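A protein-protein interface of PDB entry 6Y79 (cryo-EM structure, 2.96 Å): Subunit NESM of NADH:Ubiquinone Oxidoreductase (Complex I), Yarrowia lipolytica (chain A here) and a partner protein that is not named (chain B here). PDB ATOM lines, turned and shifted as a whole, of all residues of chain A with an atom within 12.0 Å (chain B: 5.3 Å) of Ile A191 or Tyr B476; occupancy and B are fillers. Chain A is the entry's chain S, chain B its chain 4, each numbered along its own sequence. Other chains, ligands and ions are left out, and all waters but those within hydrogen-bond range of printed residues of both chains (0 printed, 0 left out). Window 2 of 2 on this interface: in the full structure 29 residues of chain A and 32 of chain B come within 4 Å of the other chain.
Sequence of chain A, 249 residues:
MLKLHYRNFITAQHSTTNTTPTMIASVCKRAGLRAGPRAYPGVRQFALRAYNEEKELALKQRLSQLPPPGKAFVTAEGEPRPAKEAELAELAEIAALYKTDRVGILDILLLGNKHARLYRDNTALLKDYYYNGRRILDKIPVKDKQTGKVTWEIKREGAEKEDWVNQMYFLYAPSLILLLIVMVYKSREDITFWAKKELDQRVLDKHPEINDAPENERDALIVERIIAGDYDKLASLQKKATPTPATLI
The backbone carbonyl oxygen of Thr B48 lies within hydrogen-bond range of the side-chain hydroxyl of Tyr B476 (2.7 Å). The indole nitrogen (NE1) of Trp B477 is in hydrogen-bond range of the backbone carbonyl oxygen (O) of Thr B48.
Met A183 touches Asn B473. Thr B48 touches Glu A189 (OG1 to O, 3.6 Å). CG2 of Ile A191 touches CD1 of Tyr B476 (3.7 Å). Phe B49 touches Trp A194 (CZ to CE2, 3.8 Å).
Printed residues of chain B within 4 Å of Met A183: Asn B473. Of the printed residues of chain B, Ser A187 touches Asn B473. Ile A191 touches just one residue of chain B: Tyr B476 (3.7 Å). Printed residues of chain B within 4 Å of Trp A194: Phe B49 (3.8 Å). Of chain A, only Glu A189 (3.6 Å) comes within 4 Å of Thr B48. Of chain A, only Trp A194 comes within 4 Å of Phe B49. No residue of chain A comes within 4 Å of Tyr B472. Of chain A, only Ile A191 (3.7 Å) comes within 4 Å of Tyr B476. No residue of chain A comes within 4 Å of Thr B478. No residue of chain A comes within 4 Å of Val B479. The nearest printed residue of chain B that does not touch Ser A187 is Tyr B472 (5.9 Å).
ND2 of Asn B473 sits close to O of Lys A186, at 3.3 Å. The backbone NH of Ser A187 sits close to the side-chain amide nitrogen of Asn B473.
Printed residues of chain A that touch a printed residue of chain B: Met A183, Lys A186, Ser A187, Glu A189, Ile A191 and Trp A194. Of the 11 printed residues of chain B, 4 touch a printed residue of chain A. Printed residues of chain B that touch a printed residue of chain A: Thr B48, Phe B49, Asn B473 and Tyr B476. Among the printed residues, no Asp or Glu carboxylate lies within 4 Å of a Lys or Arg side-chain nitrogen of the other chain.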
ATOM      1  N   VAL A 182      11.955   7.876 -26.382  1.00  0.00           N
ATOM      2  CA  VAL A 182      10.932   8.356 -25.463  1.00  0.00           C
ATOM      3  C   VAL A 182       9.561   8.267 -26.125  1.00  0.00           C
ATOM      4  O   VAL A 182       8.589   7.899 -25.471  1.00  0.00           O
ATOM      5  CB  VAL A 182      11.241   9.779 -24.954  1.00  0.00           C
ATOM      6  CG1 VAL A 182      10.144  10.297 -24.026  1.00  0.00           C
ATOM      7  CG2 VAL A 182      12.552   9.772 -24.198  1.00  0.00           C
ATOM      8  N   MET A 183       9.465   8.489 -27.441  1.00  0.00           N
ATOM      9  CA  MET A 183       8.177   8.338 -28.123  1.00  0.00           C
ATOM     10  C   MET A 183       7.739   6.884 -28.202  1.00  0.00           C
ATOM     11  O   MET A 183       6.548   6.587 -28.071  1.00  0.00           O
ATOM     12  CB  MET A 183       8.247   8.914 -29.528  1.00  0.00           C
ATOM     13  CG  MET A 183       8.227  10.396 -29.583  1.00  0.00           C
ATOM     14  SD  MET A 183       8.437  10.978 -31.258  1.00  0.00           S
ATOM     15  CE  MET A 183       6.750  10.898 -31.803  1.00  0.00           C
ATOM     16  N   VAL A 184       8.683   5.972 -28.440  1.00  0.00           N
ATOM     17  CA  VAL A 184       8.341   4.563 -28.606  1.00  0.00           C
ATOM     18  C   VAL A 184       7.879   3.962 -27.287  1.00  0.00           C
ATOM     19  O   VAL A 184       6.847   3.282 -27.229  1.00  0.00           O
ATOM     20  CB  VAL A 184       9.537   3.794 -29.200  1.00  0.00           C
ATOM     21  CG1 VAL A 184       9.373   2.296 -29.019  1.00  0.00           C
ATOM     22  CG2 VAL A 184       9.677   4.113 -30.669  1.00  0.00           C
ATOM     23  N   TYR A 185       8.602   4.226 -26.200  1.00  0.00           N
ATOM     24  CA  TYR A 185       8.170   3.680 -24.925  1.00  0.00           C
ATOM     25  C   TYR A 185       7.105   4.516 -24.243  1.00  0.00           C
ATOM     26  O   TYR A 185       6.464   4.021 -23.312  1.00  0.00           O
ATOM     27  CB  TYR A 185       9.354   3.497 -23.985  1.00  0.00           C
ATOM     28  CG  TYR A 185      10.283   2.427 -24.463  1.00  0.00           C
ATOM     29  CD1 TYR A 185       9.918   1.095 -24.409  1.00  0.00           C
ATOM     30  CD2 TYR A 185      11.514   2.753 -24.989  1.00  0.00           C
ATOM     31  CE1 TYR A 185      10.766   0.118 -24.855  1.00  0.00           C
ATOM     32  CE2 TYR A 185      12.366   1.787 -25.438  1.00  0.00           C
ATOM     33  CZ  TYR A 185      11.988   0.475 -25.367  1.00  0.00           C
ATOM     34  OH  TYR A 185      12.847  -0.485 -25.817  1.00  0.00           O
ATOM     35  N   LYS A 186       6.889   5.757 -24.677  1.00  0.00           N
ATOM     36  CA  LYS A 186       5.762   6.519 -24.170  1.00  0.00           C
ATOM     37  C   LYS A 186       4.465   6.083 -24.838  1.00  0.00           C
ATOM     38  O   LYS A 186       3.380   6.375 -24.329  1.00  0.00           O
ATOM     39  CB  LYS A 186       6.043   8.019 -24.363  1.00  0.00           C
ATOM     40  CG  LYS A 186       5.075   8.984 -23.682  1.00  0.00           C
ATOM     41  CD  LYS A 186       5.253   9.046 -22.182  1.00  0.00           C
ATOM     42  CE  LYS A 186       6.370   9.980 -21.794  1.00  0.00           C
ATOM     43  NZ  LYS A 186       6.276  10.363 -20.363  1.00  0.00           N
ATOM     44  N   SER A 187       4.553   5.352 -25.947  1.00  0.00           N
ATOM     45  CA  SER A 187       3.364   4.876 -26.641  1.00  0.00           C
ATOM     46  C   SER A 187       2.732   3.668 -25.967  1.00  0.00           C
ATOM     47  O   SER A 187       1.621   3.287 -26.343  1.00  0.00           O
ATOM     48  CB  SER A 187       3.699   4.534 -28.087  1.00  0.00           C
ATOM     49  OG  SER A 187       2.561   4.037 -28.765  1.00  0.00           O
ATOM     50  N   ARG A 188       3.428   3.035 -25.020  1.00  0.00           N
ATOM     51  CA  ARG A 188       2.822   2.015 -24.172  1.00  0.00           C
ATOM     52  C   ARG A 188       1.655   2.606 -23.393  1.00  0.00           C
ATOM     53  O   ARG A 188       0.577   2.012 -23.292  1.00  0.00           O
ATOM     54  CB  ARG A 188       3.870   1.451 -23.210  1.00  0.00           C
ATOM     55  CG  ARG A 188       5.132   0.955 -23.872  1.00  0.00           C
ATOM     56  CD  ARG A 188       4.899  -0.396 -24.487  1.00  0.00           C
ATOM     57  NE  ARG A 188       6.077  -0.909 -25.170  1.00  0.00           N
ATOM     58  CZ  ARG A 188       6.159  -2.134 -25.674  1.00  0.00           C
ATOM     59  NH1 ARG A 188       7.267  -2.530 -26.283  1.00  0.00           N
ATOM     60  NH2 ARG A 188       5.129  -2.966 -25.570  1.00  0.00           N
ATOM     61  N   GLU A 189       1.878   3.796 -22.851  1.00  0.00           N
ATOM     62  CA  GLU A 189       0.904   4.565 -22.081  1.00  0.00           C
ATOM     63  C   GLU A 189      -0.082   5.191 -23.045  1.00  0.00           C
ATOM     64  O   GLU A 189       0.075   6.343 -23.450  1.00  0.00           O
ATOM     65  CB  GLU A 189       1.606   5.655 -21.280  1.00  0.00           C
ATOM     66  CG  GLU A 189       2.578   5.230 -20.182  1.00  0.00           C
ATOM     67  CD  GLU A 189       3.952   4.823 -20.725  1.00  0.00           C
ATOM     68  OE1 GLU A 189       4.096   4.709 -21.957  1.00  0.00           O
ATOM     69  OE2 GLU A 189       4.890   4.676 -19.929  1.00  0.00           O
ATOM     70  N   ASP A 190      -1.104   4.443 -23.450  1.00  0.00           N
ATOM     71  CA  ASP A 190      -2.176   5.071 -24.201  1.00  0.00           C
ATOM     72  C   ASP A 190      -3.531   4.489 -23.837  1.00  0.00           C
ATOM     73  O   ASP A 190      -3.644   3.518 -23.084  1.00  0.00           O
ATOM     74  CB  ASP A 190      -1.923   5.043 -25.744  1.00  0.00           C
ATOM     75  CG  ASP A 190      -1.958   3.648 -26.394  1.00  0.00           C
ATOM     76  OD1 ASP A 190      -2.784   2.755 -26.089  1.00  0.00           O
ATOM     77  OD2 ASP A 190      -1.123   3.469 -27.300  1.00  0.00           O
ATOM     78  N   ILE A 191      -4.559   5.101 -24.420  1.00  0.00           N
ATOM     79  CA  ILE A 191      -5.930   4.903 -23.983  1.00  0.00           C
ATOM     80  C   ILE A 191      -6.505   3.593 -24.509  1.00  0.00           C
ATOM     81  O   ILE A 191      -7.501   3.091 -23.984  1.00  0.00           O
ATOM     82  CB  ILE A 191      -6.753   6.132 -24.413  1.00  0.00           C
ATOM     83  CG1 ILE A 191      -8.074   6.234 -23.647  1.00  0.00           C
ATOM     84  CG2 ILE A 191      -6.927   6.145 -25.916  1.00  0.00           C
ATOM     85  CD1 ILE A 191      -7.916   6.707 -22.235  1.00  0.00           C
ATOM     86  N   THR A 192      -5.879   2.989 -25.518  1.00  0.00           N
ATOM     87  CA  THR A 192      -6.450   1.764 -26.068  1.00  0.00           C
ATOM     88  C   THR A 192      -6.061   0.536 -25.247  1.00  0.00           C
ATOM     89  O   THR A 192      -6.918  -0.312 -24.961  1.00  0.00           O
ATOM     90  CB  THR A 192      -6.036   1.606 -27.528  1.00  0.00           C
ATOM     91  OG1 THR A 192      -4.611   1.528 -27.615  1.00  0.00           O
ATOM     92  CG2 THR A 192      -6.509   2.795 -28.334  1.00  0.00           C
ATOM     93  N   PHE A 193      -4.789   0.438 -24.837  1.00  0.00           N
ATOM     94  CA  PHE A 193      -4.375  -0.615 -23.911  1.00  0.00           C
ATOM     95  C   PHE A 193      -5.073  -0.461 -22.566  1.00  0.00           C
ATOM     96  O   PHE A 193      -5.600  -1.435 -22.004  1.00  0.00           O
ATOM     97  CB  PHE A 193      -2.856  -0.591 -23.711  1.00  0.00           C
ATOM     98  CG  PHE A 193      -2.061  -0.984 -24.927  1.00  0.00           C
ATOM     99  CD1 PHE A 193      -1.911  -2.314 -25.284  1.00  0.00           C
ATOM    100  CD2 PHE A 193      -1.421  -0.019 -25.682  1.00  0.00           C
ATOM    101  CE1 PHE A 193      -1.163  -2.666 -26.400  1.00  0.00           C
ATOM    102  CE2 PHE A 193      -0.677  -0.361 -26.793  1.00  0.00           C
ATOM    103  CZ  PHE A 193      -0.547  -1.681 -27.148  1.00  0.00           C
ATOM    104  N   TRP A 194      -5.101   0.771 -22.047  1.00  0.00           N
ATOM    105  CA  TRP A 194      -5.780   1.054 -20.790  1.00  0.00           C
ATOM    106  C   TRP A 194      -7.274   0.791 -20.883  1.00  0.00           C
ATOM    107  O   TRP A 194      -7.875   0.307 -19.921  1.00  0.00           O
ATOM    108  CB  TRP A 194      -5.522   2.505 -20.370  1.00  0.00           C
ATOM    109  CG  TRP A 194      -6.234   2.882 -19.114  1.00  0.00           C
ATOM    110  CD1 TRP A 194      -5.776   2.744 -17.838  1.00  0.00           C
ATOM    111  CD2 TRP A 194      -7.542   3.444 -19.011  1.00  0.00           C
ATOM    112  NE1 TRP A 194      -6.720   3.186 -16.949  1.00  0.00           N
ATOM    113  CE2 TRP A 194      -7.816   3.615 -17.647  1.00  0.00           C
ATOM    114  CE3 TRP A 194      -8.513   3.805 -19.944  1.00  0.00           C
ATOM    115  CZ2 TRP A 194      -9.013   4.139 -17.196  1.00  0.00           C
ATOM    116  CZ3 TRP A 194      -9.696   4.319 -19.497  1.00  0.00           C
ATOM    117  CH2 TRP A 194      -9.939   4.485 -18.136  1.00  0.00           C
ATOM    118  N   ALA A 195      -7.884   1.068 -22.032  1.00  0.00           N
ATOM    119  CA  ALA A 195      -9.320   0.884 -22.174  1.00  0.00           C
ATOM    120  C   ALA A 195      -9.694  -0.579 -22.323  1.00  0.00           C
ATOM    121  O   ALA A 195     -10.753  -0.990 -21.830  1.00  0.00           O
ATOM    122  CB  ALA A 195      -9.841   1.686 -23.362  1.00  0.00           C
ATOM    123  N   LYS A 196      -8.843  -1.387 -22.962  1.00  0.00           N
ATOM    124  CA  LYS A 196      -9.117  -2.820 -22.992  1.00  0.00           C
ATOM    125  C   LYS A 196      -8.933  -3.439 -21.607  1.00  0.00           C
ATOM    126  O   LYS A 196      -9.729  -4.301 -21.196  1.00  0.00           O
ATOM    127  CB  LYS A 196      -8.263  -3.507 -24.071  1.00  0.00           C
ATOM    128  CG  LYS A 196      -6.857  -3.950 -23.711  1.00  0.00           C
ATOM    129  CD  LYS A 196      -6.130  -4.525 -24.914  1.00  0.00           C
ATOM    130  CE  LYS A 196      -5.877  -3.470 -25.979  1.00  0.00           C
ATOM    131  NZ  LYS A 196      -4.722  -3.833 -26.843  1.00  0.00           N
ATOM    132  N   LYS A 197      -7.959  -2.940 -20.830  1.00  0.00           N
ATOM    133  CA  LYS A 197      -7.793  -3.441 -19.469  1.00  0.00           C
ATOM    134  C   LYS A 197      -8.940  -2.996 -18.572  1.00  0.00           C
ATOM    135  O   LYS A 197      -9.376  -3.751 -17.697  1.00  0.00           O
ATOM    136  CB  LYS A 197      -6.453  -2.992 -18.898  1.00  0.00           C
ATOM    137  CG  LYS A 197      -5.280  -3.706 -19.517  1.00  0.00           C
ATOM    138  CD  LYS A 197      -3.968  -3.186 -18.985  1.00  0.00           C
ATOM    139  CE  LYS A 197      -3.777  -3.573 -17.535  1.00  0.00           C
ATOM    140  NZ  LYS A 197      -2.460  -3.112 -17.028  1.00  0.00           N
ATOM    141  N   GLU A 198      -9.482  -1.802 -18.815  1.00  0.00           N
ATOM    142  CA  GLU A 198     -10.606  -1.318 -18.023  1.00  0.00           C
ATOM    143  C   GLU A 198     -11.887  -2.078 -18.340  1.00  0.00           C
ATOM    144  O   GLU A 198     -12.662  -2.389 -17.433  1.00  0.00           O
ATOM    145  CB  GLU A 198     -10.798   0.180 -18.248  1.00  0.00           C
ATOM    146  CG  GLU A 198     -11.975   0.790 -17.496  1.00  0.00           C
ATOM    147  CD  GLU A 198     -11.740   0.852 -16.003  1.00  0.00           C
ATOM    148  OE1 GLU A 198     -10.568   0.973 -15.599  1.00  0.00           O
ATOM    149  OE2 GLU A 198     -12.722   0.780 -15.236  1.00  0.00           O
ATOM    150  N   LEU A 199     -12.120  -2.396 -19.616  1.00  0.00           N
ATOM    151  CA  LEU A 199     -13.315  -3.151 -19.991  1.00  0.00           C
ATOM    152  C   LEU A 199     -13.267  -4.579 -19.449  1.00  0.00           C
ATOM    153  O   LEU A 199     -14.285  -5.105 -18.965  1.00  0.00           O
ATOM    154  CB  LEU A 199     -13.456  -3.140 -21.509  1.00  0.00           C
ATOM    155  CG  LEU A 199     -14.688  -3.712 -22.196  1.00  0.00           C
ATOM    156  CD1 LEU A 199     -15.941  -3.042 -21.701  1.00  0.00           C
ATOM    157  CD2 LEU A 199     -14.552  -3.522 -23.688  1.00  0.00           C
ATOM    158  N   ASP A 200     -12.080  -5.204 -19.498  1.00  0.00           N
ATOM    159  CA  ASP A 200     -11.871  -6.497 -18.848  1.00  0.00           C
ATOM    160  C   ASP A 200     -12.108  -6.413 -17.346  1.00  0.00           C
ATOM    161  O   ASP A 200     -12.747  -7.301 -16.765  1.00  0.00           O
ATOM    162  CB  ASP A 200     -10.449  -6.995 -19.134  1.00  0.00           C
ATOM    163  CG  ASP A 200     -10.253  -8.483 -18.827  1.00  0.00           C
ATOM    164  OD1 ASP A 200     -11.164  -9.125 -18.262  1.00  0.00           O
ATOM    165  OD2 ASP A 200      -9.205  -9.031 -19.209  1.00  0.00           O
ATOM    166  N   GLN A 201     -11.591  -5.357 -16.707  1.00  0.00           N
ATOM    167  CA  GLN A 201     -11.777  -5.193 -15.271  1.00  0.00           C
ATOM    168  C   GLN A 201     -13.245  -4.997 -14.922  1.00  0.00           C
ATOM    169  O   GLN A 201     -13.709  -5.483 -13.893  1.00  0.00           O
ATOM    170  CB  GLN A 201     -10.945  -4.023 -14.771  1.00  0.00           C
ATOM    171  CG  GLN A 201     -10.974  -3.829 -13.266  1.00  0.00           C
ATOM    172  CD  GLN A 201     -10.463  -5.039 -12.517  1.00  0.00           C
ATOM    173  OE1 GLN A 201     -11.237  -5.789 -11.924  1.00  0.00           O
ATOM    174  NE2 GLN A 201      -9.152  -5.231 -12.531  1.00  0.00           N
ATOM    175  N   ARG A 202     -14.006  -4.345 -15.800  1.00  0.00           N
ATOM    176  CA  ARG A 202     -15.423  -4.125 -15.525  1.00  0.00           C
ATOM    177  C   ARG A 202     -16.232  -5.410 -15.644  1.00  0.00           C
ATOM    178  O   ARG A 202     -17.164  -5.639 -14.858  1.00  0.00           O
ATOM    179  CB  ARG A 202     -15.979  -3.058 -16.461  1.00  0.00           C
ATOM    180  CG  ARG A 202     -15.560  -1.663 -16.090  1.00  0.00           C
ATOM    181  CD  ARG A 202     -16.196  -0.648 -16.999  1.00  0.00           C
ATOM    182  NE  ARG A 202     -15.653   0.685 -16.779  1.00  0.00           N
ATOM    183  CZ  ARG A 202     -16.057   1.766 -17.431  1.00  0.00           C
ATOM    184  NH1 ARG A 202     -17.011   1.672 -18.344  1.00  0.00           N
ATOM    185  NH2 ARG A 202     -15.509   2.943 -17.172  1.00  0.00           N
ATOM    186  N   THR B  48       0.620  11.943 -20.232  1.00  0.00           N
ATOM    187  CA  THR B  48      -0.293  11.757 -21.347  1.00  0.00           C
ATOM    188  C   THR B  48      -1.696  11.395 -20.893  1.00  0.00           C
ATOM    189  O   THR B  48      -2.640  11.525 -21.678  1.00  0.00           O
ATOM    190  CB  THR B  48       0.241  10.675 -22.278  1.00  0.00           C
ATOM    191  OG1 THR B  48       0.226   9.416 -21.599  1.00  0.00           O
ATOM    192  CG2 THR B  48       1.662  10.995 -22.690  1.00  0.00           C
ATOM    193  N   PHE B  49      -1.856  10.964 -19.646  1.00  0.00           N
ATOM    194  CA  PHE B  49      -3.152  10.563 -19.117  1.00  0.00           C
ATOM    195  C   PHE B  49      -3.995  11.745 -18.658  1.00  0.00           C
ATOM    196  O   PHE B  49      -5.114  11.542 -18.179  1.00  0.00           O
ATOM    197  CB  PHE B  49      -2.952   9.579 -17.965  1.00  0.00           C
ATOM    198  CG  PHE B  49      -4.125   8.681 -17.723  1.00  0.00           C
ATOM    199  CD1 PHE B  49      -4.543   7.792 -18.694  1.00  0.00           C
ATOM    200  CD2 PHE B  49      -4.810   8.730 -16.524  1.00  0.00           C
ATOM    201  CE1 PHE B  49      -5.623   6.968 -18.474  1.00  0.00           C
ATOM    202  CE2 PHE B  49      -5.893   7.905 -16.300  1.00  0.00           C
ATOM    203  CZ  PHE B  49      -6.298   7.024 -17.276  1.00  0.00           C
ATOM    204  N   TYR B 472       0.624   9.080 -31.350  1.00  0.00           N
ATOM    205  CA  TYR B 472      -0.764   9.048 -30.920  1.00  0.00           C
ATOM    206  C   TYR B 472      -0.905   9.325 -29.432  1.00  0.00           C
ATOM    207  O   TYR B 472      -1.942   9.845 -29.012  1.00  0.00           O
ATOM    208  CB  TYR B 472      -1.383   7.702 -31.268  1.00  0.00           C
ATOM    209  CG  TYR B 472      -2.863   7.600 -31.013  1.00  0.00           C
ATOM    210  CD1 TYR B 472      -3.750   8.491 -31.591  1.00  0.00           C
ATOM    211  CD2 TYR B 472      -3.376   6.585 -30.225  1.00  0.00           C
ATOM    212  CE1 TYR B 472      -5.102   8.388 -31.371  1.00  0.00           C
ATOM    213  CE2 TYR B 472      -4.723   6.471 -30.005  1.00  0.00           C
ATOM    214  CZ  TYR B 472      -5.580   7.373 -30.580  1.00  0.00           C
ATOM    215  OH  TYR B 472      -6.927   7.256 -30.356  1.00  0.00           O
ATOM    216  N   ASN B 473       0.129   9.030 -28.637  1.00  0.00           N
ATOM    217  CA  ASN B 473       0.079   9.207 -27.190  1.00  0.00           C
ATOM    218  C   ASN B 473      -0.057  10.664 -26.774  1.00  0.00           C
ATOM    219  O   ASN B 473      -0.483  10.943 -25.650  1.00  0.00           O
ATOM    220  CB  ASN B 473       1.333   8.616 -26.548  1.00  0.00           C
ATOM    221  CG  ASN B 473       2.610   9.097 -27.203  1.00  0.00           C
ATOM    222  OD1 ASN B 473       2.596   9.946 -28.082  1.00  0.00           O
ATOM    223  ND2 ASN B 473       3.722   8.550 -26.775  1.00  0.00           N
ATOM    224  N   LEU B 474       0.320  11.589 -27.641  1.00  0.00           N
ATOM    225  CA  LEU B 474       0.099  12.999 -27.396  1.00  0.00           C
ATOM    226  C   LEU B 474      -1.268  13.455 -27.852  1.00  0.00           C
ATOM    227  O   LEU B 474      -1.811  14.415 -27.302  1.00  0.00           O
ATOM    228  CB  LEU B 474       1.164  13.820 -28.108  1.00  0.00           C
ATOM    229  CG  LEU B 474       2.557  13.572 -27.560  1.00  0.00           C
ATOM    230  CD1 LEU B 474       3.596  14.232 -28.428  1.00  0.00           C
ATOM    231  CD2 LEU B 474       2.589  14.129 -26.172  1.00  0.00           C
ATOM    232  N   LEU B 475      -1.853  12.778 -28.828  1.00  0.00           N
ATOM    233  CA  LEU B 475      -2.945  13.384 -29.559  1.00  0.00           C
ATOM    234  C   LEU B 475      -4.306  12.796 -29.250  1.00  0.00           C
ATOM    235  O   LEU B 475      -5.305  13.393 -29.656  1.00  0.00           O
ATOM    236  CB  LEU B 475      -2.686  13.275 -31.059  1.00  0.00           C
ATOM    237  CG  LEU B 475      -1.464  14.042 -31.546  1.00  0.00           C
ATOM    238  CD1 LEU B 475      -1.263  13.755 -33.010  1.00  0.00           C
ATOM    239  CD2 LEU B 475      -1.634  15.525 -31.303  1.00  0.00           C
ATOM    240  N   TYR B 476      -4.381  11.675 -28.524  1.00  0.00           N
ATOM    241  CA  TYR B 476      -5.652  10.970 -28.392  1.00  0.00           C
ATOM    242  C   TYR B 476      -6.674  11.744 -27.578  1.00  0.00           C
ATOM    243  O   TYR B 476      -7.877  11.514 -27.736  1.00  0.00           O
ATOM    244  CB  TYR B 476      -5.442   9.574 -27.798  1.00  0.00           C
ATOM    245  CG  TYR B 476      -4.887   9.486 -26.397  1.00  0.00           C
ATOM    246  CD1 TYR B 476      -5.721   9.536 -25.285  1.00  0.00           C
ATOM    247  CD2 TYR B 476      -3.536   9.278 -26.186  1.00  0.00           C
ATOM    248  CE1 TYR B 476      -5.219   9.430 -24.019  1.00  0.00           C
ATOM    249  CE2 TYR B 476      -3.027   9.166 -24.917  1.00  0.00           C
ATOM    250  CZ  TYR B 476      -3.872   9.244 -23.840  1.00  0.00           C
ATOM    251  OH  TYR B 476      -3.369   9.132 -22.569  1.00  0.00           O
ATOM    252  N   TRP B 477      -6.229  12.655 -26.716  1.00  0.00           N
ATOM    253  CA  TRP B 477      -7.153  13.603 -26.117  1.00  0.00           C
ATOM    254  C   TRP B 477      -7.621  14.604 -27.152  1.00  0.00           C
ATOM    255  O   TRP B 477      -8.824  14.759 -27.382  1.00  0.00           O
ATOM    256  CB  TRP B 477      -6.491  14.328 -24.948  1.00  0.00           C
ATOM    257  CG  TRP B 477      -6.163  13.458 -23.805  1.00  0.00           C
ATOM    258  CD1 TRP B 477      -4.930  13.059 -23.419  1.00  0.00           C
ATOM    259  CD2 TRP B 477      -7.082  12.870 -22.887  1.00  0.00           C
ATOM    260  NE1 TRP B 477      -5.017  12.259 -22.313  1.00  0.00           N
ATOM    261  CE2 TRP B 477      -6.334  12.126 -21.969  1.00  0.00           C
ATOM    262  CE3 TRP B 477      -8.469  12.899 -22.755  1.00  0.00           C
ATOM    263  CZ2 TRP B 477      -6.919  11.419 -20.931  1.00  0.00           C
ATOM    264  CZ3 TRP B 477      -9.046  12.201 -21.721  1.00  0.00           C
ATOM    265  CH2 TRP B 477      -8.276  11.468 -20.828  1.00  0.00           C
ATOM    266  N   THR B 478      -6.675  15.262 -27.820  1.00  0.00           N
ATOM    267  CA  THR B 478      -6.968  16.397 -28.683  1.00  0.00           C
ATOM    268  C   THR B 478      -7.642  15.997 -29.978  1.00  0.00           C
ATOM    269  O   THR B 478      -8.109  16.865 -30.714  1.00  0.00           O
ATOM    270  CB  THR B 478      -5.682  17.158 -28.991  1.00  0.00           C
ATOM    271  OG1 THR B 478      -4.823  16.342 -29.788  1.00  0.00           O
ATOM    272  CG2 THR B 478      -4.967  17.502 -27.700  1.00  0.00           C
ATOM    273  N   VAL B 479      -7.695  14.708 -30.267  1.00  0.00           N
ATOM    274  CA  VAL B 479      -8.428  14.207 -31.410  1.00  0.00           C
ATOM    275  C   VAL B 479      -9.907  14.071 -31.057  1.00  0.00           C
ATOM    276  O   VAL B 479     -10.781  14.251 -31.914  1.00  0.00           O
ATOM    277  CB  VAL B 479      -7.733  12.904 -31.845  1.00  0.00           C
ATOM    278  CG1 VAL B 479      -8.615  11.992 -32.587  1.00  0.00           C
ATOM    279  CG2 VAL B 479      -6.522  13.241 -32.699  1.00  0.00           C
ATOM    280  N   ASN B 480     -10.213  13.855 -29.774  1.00  0.00           N
ATOM    281  CA  ASN B 480     -11.590  13.854 -29.292  1.00  0.00           C
ATOM    282  C   ASN B 480     -12.060  15.236 -28.841  1.00  0.00           C
ATOM    283  O   ASN B 480     -13.267  15.462 -28.731  1.00  0.00           O
ATOM    284  CB  ASN B 480     -11.728  12.860 -28.139  1.00  0.00           C
ATOM    285  CG  ASN B 480     -13.160  12.444 -27.893  1.00  0.00           C
ATOM    286  OD1 ASN B 480     -14.036  12.674 -28.717  1.00  0.00           O
ATOM    287  ND2 ASN B 480     -13.406  11.848 -26.744  1.00  0.00           N
